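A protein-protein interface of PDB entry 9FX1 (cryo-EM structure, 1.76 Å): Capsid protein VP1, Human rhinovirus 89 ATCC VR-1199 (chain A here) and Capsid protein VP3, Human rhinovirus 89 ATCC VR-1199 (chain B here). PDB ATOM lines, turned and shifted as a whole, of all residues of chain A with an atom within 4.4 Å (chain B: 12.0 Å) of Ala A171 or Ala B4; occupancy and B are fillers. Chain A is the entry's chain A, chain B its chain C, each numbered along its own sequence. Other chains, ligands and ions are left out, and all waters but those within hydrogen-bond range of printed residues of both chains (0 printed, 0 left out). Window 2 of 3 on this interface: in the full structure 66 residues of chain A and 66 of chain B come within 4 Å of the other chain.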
ATOM      1  N   PHE A 147      20.318 -31.890  14.828  1.00  0.00           N
ATOM      2  CA  PHE A 147      19.856 -30.652  14.206  1.00  0.00           C
ATOM      3  C   PHE A 147      19.538 -29.681  15.330  1.00  0.00           C
ATOM      4  O   PHE A 147      18.694 -29.976  16.168  1.00  0.00           O
ATOM      5  CB  PHE A 147      18.590 -30.910  13.383  1.00  0.00           C
ATOM      6  CG  PHE A 147      18.786 -31.924  12.286  1.00  0.00           C
ATOM      7  CD1 PHE A 147      18.653 -33.296  12.559  1.00  0.00           C
ATOM      8  CD2 PHE A 147      19.135 -31.488  10.998  1.00  0.00           C
ATOM      9  CE1 PHE A 147      18.905 -34.237  11.548  1.00  0.00           C
ATOM     10  CE2 PHE A 147      19.379 -32.429   9.989  1.00  0.00           C
ATOM     11  CZ  PHE A 147      19.287 -33.802  10.269  1.00  0.00           C
ATOM     12  N   MET A 148      20.194 -28.535  15.359  1.00  0.00           N
ATOM     13  CA  MET A 148      20.004 -27.512  16.371  1.00  0.00           C
ATOM     14  C   MET A 148      19.478 -26.247  15.708  1.00  0.00           C
ATOM     15  O   MET A 148      20.103 -25.730  14.785  1.00  0.00           O
ATOM     16  CB  MET A 148      21.328 -27.277  17.104  1.00  0.00           C
ATOM     17  CG  MET A 148      21.176 -26.228  18.206  1.00  0.00           C
ATOM     18  SD  MET A 148      22.609 -26.109  19.306  1.00  0.00           S
ATOM     19  CE  MET A 148      23.905 -25.657  18.117  1.00  0.00           C
ATOM     20  N   TYR A 149      18.337 -25.743  16.165  1.00  0.00           N
ATOM     21  CA  TYR A 149      17.876 -24.430  15.745  1.00  0.00           C
ATOM     22  C   TYR A 149      18.570 -23.357  16.581  1.00  0.00           C
ATOM     23  O   TYR A 149      18.426 -23.331  17.800  1.00  0.00           O
ATOM     24  CB  TYR A 149      16.360 -24.311  15.854  1.00  0.00           C
ATOM     25  CG  TYR A 149      15.910 -22.916  15.485  1.00  0.00           C
ATOM     26  CD1 TYR A 149      16.113 -22.455  14.174  1.00  0.00           C
ATOM     27  CD2 TYR A 149      15.389 -22.055  16.468  1.00  0.00           C
ATOM     28  CE1 TYR A 149      15.751 -21.143  13.829  1.00  0.00           C
ATOM     29  CE2 TYR A 149      15.022 -20.741  16.123  1.00  0.00           C
ATOM     30  CZ  TYR A 149      15.202 -20.287  14.805  1.00  0.00           C
ATOM     31  OH  TYR A 149      14.871 -19.015  14.484  1.00  0.00           O
ATOM     32  N   SER A 167      23.339 -27.423  23.670  1.00  0.00           N
ATOM     33  CA  SER A 167      21.920 -27.125  23.455  1.00  0.00           C
ATOM     34  C   SER A 167      21.149 -26.877  24.759  1.00  0.00           C
ATOM     35  O   SER A 167      19.997 -27.282  24.895  1.00  0.00           O
ATOM     36  CB  SER A 167      21.292 -28.215  22.581  1.00  0.00           C
ATOM     37  OG  SER A 167      20.106 -27.759  21.968  1.00  0.00           O
ATOM     38  N   THR A 169      19.715 -24.330  25.931  1.00  0.00           N
ATOM     39  CA  THR A 169      18.531 -23.472  25.722  1.00  0.00           C
ATOM     40  C   THR A 169      17.949 -23.581  24.307  1.00  0.00           C
ATOM     41  O   THR A 169      16.728 -23.566  24.149  1.00  0.00           O
ATOM     42  CB  THR A 169      18.875 -22.013  26.069  1.00  0.00           C
ATOM     43  OG1 THR A 169      19.426 -21.929  27.366  1.00  0.00           O
ATOM     44  CG2 THR A 169      17.662 -21.091  26.048  1.00  0.00           C
ATOM     45  N   ASN A 170      18.783 -23.745  23.274  1.00  0.00           N
ATOM     46  CA  ASN A 170      18.313 -24.003  21.907  1.00  0.00           C
ATOM     47  C   ASN A 170      17.512 -25.312  21.813  1.00  0.00           C
ATOM     48  O   ASN A 170      17.806 -26.290  22.501  1.00  0.00           O
ATOM     49  CB  ASN A 170      19.503 -24.089  20.938  1.00  0.00           C
ATOM     50  CG  ASN A 170      20.265 -22.794  20.757  1.00  0.00           C
ATOM     51  OD1 ASN A 170      19.823 -21.708  21.098  1.00  0.00           O
ATOM     52  ND2 ASN A 170      21.461 -22.905  20.240  1.00  0.00           N
ATOM     53  N   ALA A 171      16.550 -25.365  20.892  1.00  0.00           N
ATOM     54  CA  ALA A 171      15.941 -26.622  20.492  1.00  0.00           C
ATOM     55  C   ALA A 171      16.937 -27.441  19.652  1.00  0.00           C
ATOM     56  O   ALA A 171      17.446 -26.959  18.642  1.00  0.00           O
ATOM     57  CB  ALA A 171      14.655 -26.332  19.712  1.00  0.00           C
ATOM     58  N   SER A 172      17.167 -28.693  20.043  1.00  0.00           N
ATOM     59  CA  SER A 172      17.826 -29.695  19.198  1.00  0.00           C
ATOM     60  C   SER A 172      16.912 -30.897  18.992  1.00  0.00           C
ATOM     61  O   SER A 172      16.165 -31.271  19.894  1.00  0.00           O
ATOM     62  CB  SER A 172      19.153 -30.194  19.780  1.00  0.00           C
ATOM     63  OG  SER A 172      20.169 -29.223  19.698  1.00  0.00           O
ATOM     64  N   PHE A 184       8.883 -31.715  13.913  1.00  0.00           N
ATOM     65  CA  PHE A 184       8.527 -30.785  14.986  1.00  0.00           C
ATOM     66  C   PHE A 184       7.797 -29.580  14.397  1.00  0.00           C
ATOM     67  O   PHE A 184       7.884 -29.301  13.204  1.00  0.00           O
ATOM     68  CB  PHE A 184       9.783 -30.368  15.766  1.00  0.00           C
ATOM     69  CG  PHE A 184      10.870 -29.754  14.906  1.00  0.00           C
ATOM     70  CD1 PHE A 184      10.869 -28.375  14.622  1.00  0.00           C
ATOM     71  CD2 PHE A 184      11.883 -30.574  14.375  1.00  0.00           C
ATOM     72  CE1 PHE A 184      11.869 -27.825  13.799  1.00  0.00           C
ATOM     73  CE2 PHE A 184      12.872 -30.024  13.550  1.00  0.00           C
ATOM     74  CZ  PHE A 184      12.868 -28.650  13.264  1.00  0.00           C
ATOM     75  N   THR A 185       7.057 -28.860  15.231  1.00  0.00           N
ATOM     76  CA  THR A 185       6.412 -27.604  14.848  1.00  0.00           C
ATOM     77  C   THR A 185       7.247 -26.416  15.317  1.00  0.00           C
ATOM     78  O   THR A 185       7.703 -26.392  16.456  1.00  0.00           O
ATOM     79  CB  THR A 185       4.985 -27.525  15.395  1.00  0.00           C
ATOM     80  OG1 THR A 185       4.180 -28.502  14.766  1.00  0.00           O
ATOM     81  CG2 THR A 185       4.333 -26.174  15.119  1.00  0.00           C
ATOM     82  N   ILE A 186       7.398 -25.405  14.473  1.00  0.00           N
ATOM     83  CA  ILE A 186       7.817 -24.056  14.850  1.00  0.00           C
ATOM     84  C   ILE A 186       6.542 -23.196  14.848  1.00  0.00           C
ATOM     85  O   ILE A 186       5.860 -23.141  13.823  1.00  0.00           O
ATOM     86  CB  ILE A 186       8.865 -23.539  13.843  1.00  0.00           C
ATOM     87  CG1 ILE A 186      10.153 -24.381  13.837  1.00  0.00           C
ATOM     88  CG2 ILE A 186       9.202 -22.056  14.053  1.00  0.00           C
ATOM     89  CD1 ILE A 186      11.058 -24.201  15.059  1.00  0.00           C
ATOM     90  N   SER B   1       2.246 -32.912  16.144  1.00  0.00           N
ATOM     91  CA  SER B   1       3.723 -32.940  16.351  1.00  0.00           C
ATOM     92  C   SER B   1       4.166 -31.941  17.428  1.00  0.00           C
ATOM     93  O   SER B   1       3.575 -30.865  17.545  1.00  0.00           O
ATOM     94  CB  SER B   1       4.505 -32.681  15.051  1.00  0.00           C
ATOM     95  OG  SER B   1       4.269 -31.380  14.530  1.00  0.00           O
ATOM     96  N   PRO B   2       5.203 -32.253  18.223  1.00  0.00           N
ATOM     97  CA  PRO B   2       5.632 -31.409  19.342  1.00  0.00           C
ATOM     98  C   PRO B   2       6.190 -30.070  18.852  1.00  0.00           C
ATOM     99  O   PRO B   2       6.819 -30.001  17.799  1.00  0.00           O
ATOM    100  CB  PRO B   2       6.687 -32.220  20.098  1.00  0.00           C
ATOM    101  CG  PRO B   2       7.255 -33.149  19.029  1.00  0.00           C
ATOM    102  CD  PRO B   2       6.048 -33.440  18.140  1.00  0.00           C
ATOM    103  N   SER B   3       5.930 -28.991  19.587  1.00  0.00           N
ATOM    104  CA  SER B   3       6.524 -27.682  19.311  1.00  0.00           C
ATOM    105  C   SER B   3       7.981 -27.654  19.770  1.00  0.00           C
ATOM    106  O   SER B   3       8.274 -28.042  20.899  1.00  0.00           O
ATOM    107  CB  SER B   3       5.742 -26.563  20.002  1.00  0.00           C
ATOM    108  OG  SER B   3       6.319 -25.308  19.714  1.00  0.00           O
ATOM    109  N   ALA B   4       8.887 -27.145  18.941  1.00  0.00           N
ATOM    110  CA  ALA B   4      10.270 -26.905  19.342  1.00  0.00           C
ATOM    111  C   ALA B   4      10.403 -25.743  20.357  1.00  0.00           C
ATOM    112  O   ALA B   4      11.418 -25.666  21.045  1.00  0.00           O
ATOM    113  CB  ALA B   4      11.088 -26.647  18.075  1.00  0.00           C
ATOM    114  N   PHE B   5       9.401 -24.857  20.471  1.00  0.00           N
ATOM    115  CA  PHE B   5       9.402 -23.683  21.369  1.00  0.00           C
ATOM    116  C   PHE B   5       8.277 -23.794  22.434  1.00  0.00           C
ATOM    117  O   PHE B   5       7.225 -23.173  22.276  1.00  0.00           O
ATOM    118  CB  PHE B   5       9.244 -22.379  20.551  1.00  0.00           C
ATOM    119  CG  PHE B   5      10.157 -22.066  19.380  1.00  0.00           C
ATOM    120  CD1 PHE B   5      11.368 -22.742  19.144  1.00  0.00           C
ATOM    121  CD2 PHE B   5       9.773 -21.020  18.521  1.00  0.00           C
ATOM    122  CE1 PHE B   5      12.143 -22.426  18.016  1.00  0.00           C
ATOM    123  CE2 PHE B   5      10.556 -20.694  17.404  1.00  0.00           C
ATOM    124  CZ  PHE B   5      11.731 -21.412  17.141  1.00  0.00           C
ATOM    125  N   PRO B   6       8.434 -24.594  23.504  1.00  0.00           N
ATOM    126  CA  PRO B   6       7.328 -25.157  24.310  1.00  0.00           C
ATOM    127  C   PRO B   6       6.465 -24.226  25.190  1.00  0.00           C
ATOM    128  O   PRO B   6       5.479 -24.695  25.760  1.00  0.00           O
ATOM    129  CB  PRO B   6       7.982 -26.244  25.176  1.00  0.00           C
ATOM    130  CG  PRO B   6       9.449 -25.850  25.230  1.00  0.00           C
ATOM    131  CD  PRO B   6       9.680 -25.261  23.848  1.00  0.00           C
ATOM    132  N   TYR B   7       6.797 -22.945  25.338  1.00  0.00           N
ATOM    133  CA  TYR B   7       5.957 -21.963  26.065  1.00  0.00           C
ATOM    134  C   TYR B   7       5.728 -20.675  25.254  1.00  0.00           C
ATOM    135  O   TYR B   7       5.208 -19.680  25.758  1.00  0.00           O
ATOM    136  CB  TYR B   7       6.556 -21.673  27.447  1.00  0.00           C
ATOM    137  CG  TYR B   7       6.560 -22.872  28.378  1.00  0.00           C
ATOM    138  CD1 TYR B   7       5.441 -23.131  29.193  1.00  0.00           C
ATOM    139  CD2 TYR B   7       7.670 -23.735  28.418  1.00  0.00           C
ATOM    140  CE1 TYR B   7       5.427 -24.260  30.036  1.00  0.00           C
ATOM    141  CE2 TYR B   7       7.652 -24.873  29.246  1.00  0.00           C
ATOM    142  CZ  TYR B   7       6.531 -25.138  30.056  1.00  0.00           C
ATOM    143  OH  TYR B   7       6.515 -26.241  30.854  1.00  0.00           O
ATOM    144  N   PHE B   8       6.141 -20.686  23.991  1.00  0.00           N
ATOM    145  CA  PHE B   8       6.147 -19.518  23.127  1.00  0.00           C
ATOM    146  C   PHE B   8       4.729 -19.029  22.827  1.00  0.00           C
ATOM    147  O   PHE B   8       3.885 -19.811  22.391  1.00  0.00           O
ATOM    148  CB  PHE B   8       6.892 -19.915  21.856  1.00  0.00           C
ATOM    149  CG  PHE B   8       7.040 -18.804  20.853  1.00  0.00           C
ATOM    150  CD1 PHE B   8       8.158 -17.954  20.905  1.00  0.00           C
ATOM    151  CD2 PHE B   8       6.064 -18.625  19.863  1.00  0.00           C
ATOM    152  CE1 PHE B   8       8.295 -16.918  19.967  1.00  0.00           C
ATOM    153  CE2 PHE B   8       6.210 -17.599  18.919  1.00  0.00           C
ATOM    154  CZ  PHE B   8       7.316 -16.737  18.979  1.00  0.00           C
ATOM    155  N   HIS B   9       4.475 -17.735  23.004  1.00  0.00           N
ATOM    156  CA  HIS B   9       3.208 -17.090  22.659  1.00  0.00           C
ATOM    157  C   HIS B   9       3.390 -16.243  21.387  1.00  0.00           C
ATOM    158  O   HIS B   9       4.096 -15.235  21.437  1.00  0.00           O
ATOM    159  CB  HIS B   9       2.756 -16.235  23.849  1.00  0.00           C
ATOM    160  CG  HIS B   9       1.414 -15.596  23.620  1.00  0.00           C
ATOM    161  ND1 HIS B   9       0.184 -16.253  23.686  1.00  0.00           N
ATOM    162  CD2 HIS B   9       1.195 -14.287  23.308  1.00  0.00           C
ATOM    163  CE1 HIS B   9      -0.751 -15.320  23.421  1.00  0.00           C
ATOM    164  NE2 HIS B   9      -0.168 -14.133  23.194  1.00  0.00           N
ATOM    165  N   PRO B  10       2.797 -16.626  20.240  1.00  0.00           N
ATOM    166  CA  PRO B  10       2.935 -15.868  18.997  1.00  0.00           C
ATOM    167  C   PRO B  10       2.462 -14.417  19.128  1.00  0.00           C
ATOM    168  O   PRO B  10       1.542 -14.117  19.889  1.00  0.00           O
ATOM    169  CB  PRO B  10       2.107 -16.628  17.955  1.00  0.00           C
ATOM    170  CG  PRO B  10       2.093 -18.059  18.484  1.00  0.00           C
ATOM    171  CD  PRO B  10       2.059 -17.857  19.997  1.00  0.00           C
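The backbone carbonyl oxygen of Ala A171 is in hydrogen-bond range of the backbone NH of Tyr A149 (2.9 Å). The side-chain hydroxyl (OG) of Ser B3 is in hydrogen-bond range of the backbone NH (N) of Phe B5, at 3.2 Å.
Hydrophobic or aromatic side chains of chain A within 4 Å of the printed part of chain B: Tyr A149, Ala A171, Phe A184 and Ile A186. Printed residues of chain B that touch a printed residue of chain A: Ser B1, Pro B2, Ser B3, Ala B4 and Phe B5. Among the printed residues, no Asp or Glu carboxylate lies within 4 Å of a Lys or Arg side-chain nitrogen of the other chain.
The side-chain hydroxyl of Thr A185 is in hydrogen-bond range of the side-chain hydroxyl of Ser B1, 2.9 Å away. O of Pro B2 sits at hydrogen-bond distance from N of Thr A185, 2.8 Å away. The backbone carbonyl oxygen (O) of Thr A185 sits at hydrogen-bond distance from the backbone NH (N) of Ala B4 (2.9 Å).
Among the printed residues, pairs that only touch across the chains: Thr A185 with Ser B3, Phe A184 with Pro B2, Tyr A149 with Phe B5, Ile A186 with Phe B5, Ala A171 with Ala B4, Phe A184 with Ala B4, Ile A186 with Ala B4 and Phe A184 with Ser B1.
Ala A171 touches just one residue of chain B: Ala B4. No residue of chain B comes within 4 Å of Ser A167. No residue of chain B comes within 4 Å of Thr A169. No residue of chain B comes within 4 Å of Asn A170. No residue of chain B comes within 4 Å of Ser A172. Phe A184 touches just these residues of chain B: Ser B1 (3.96 Å), Pro B2 (3.4 Å) and Ala B4 (3.9 Å). Of chain B, only Ser B1 (2.9 Å), Pro B2 (2.8 Å), Ser B3 (3.3 Å) and Ala B4 (2.9 Å) come within 4 Å of Thr A185. Of chain B, only Ala B4 (3.9 Å) and Phe B5 (3.5 Å) come within 4 Å of Ile A186. Printed residues of chain A within 4 Å of Pro B2: Phe A184 (3.4 Å) and Thr A185 (2.8 Å). Printed residues of chain A within 4 Å of Ser B3: Thr A185 (3.3 Å). Printed residues of chain A within 4 Å of Phe B5: Tyr A149 (3.5 Å) and Ile A186 (3.5 Å). Printed residues of chain A within 4 Å of Ser B1: Phe A184 and Thr A185. Phe A147 touches none of the printed residues of chain B. The nearest residue of chain B that does not touch Ala A171 is Phe B5 (4.9 Å). The nearest printed residue of chain A that does not touch Ala B4 is Asn A170 (6.2 Å). The nearest printed residue of chain B that does not touch Tyr A149 is Ala B4 (6.2 Å).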
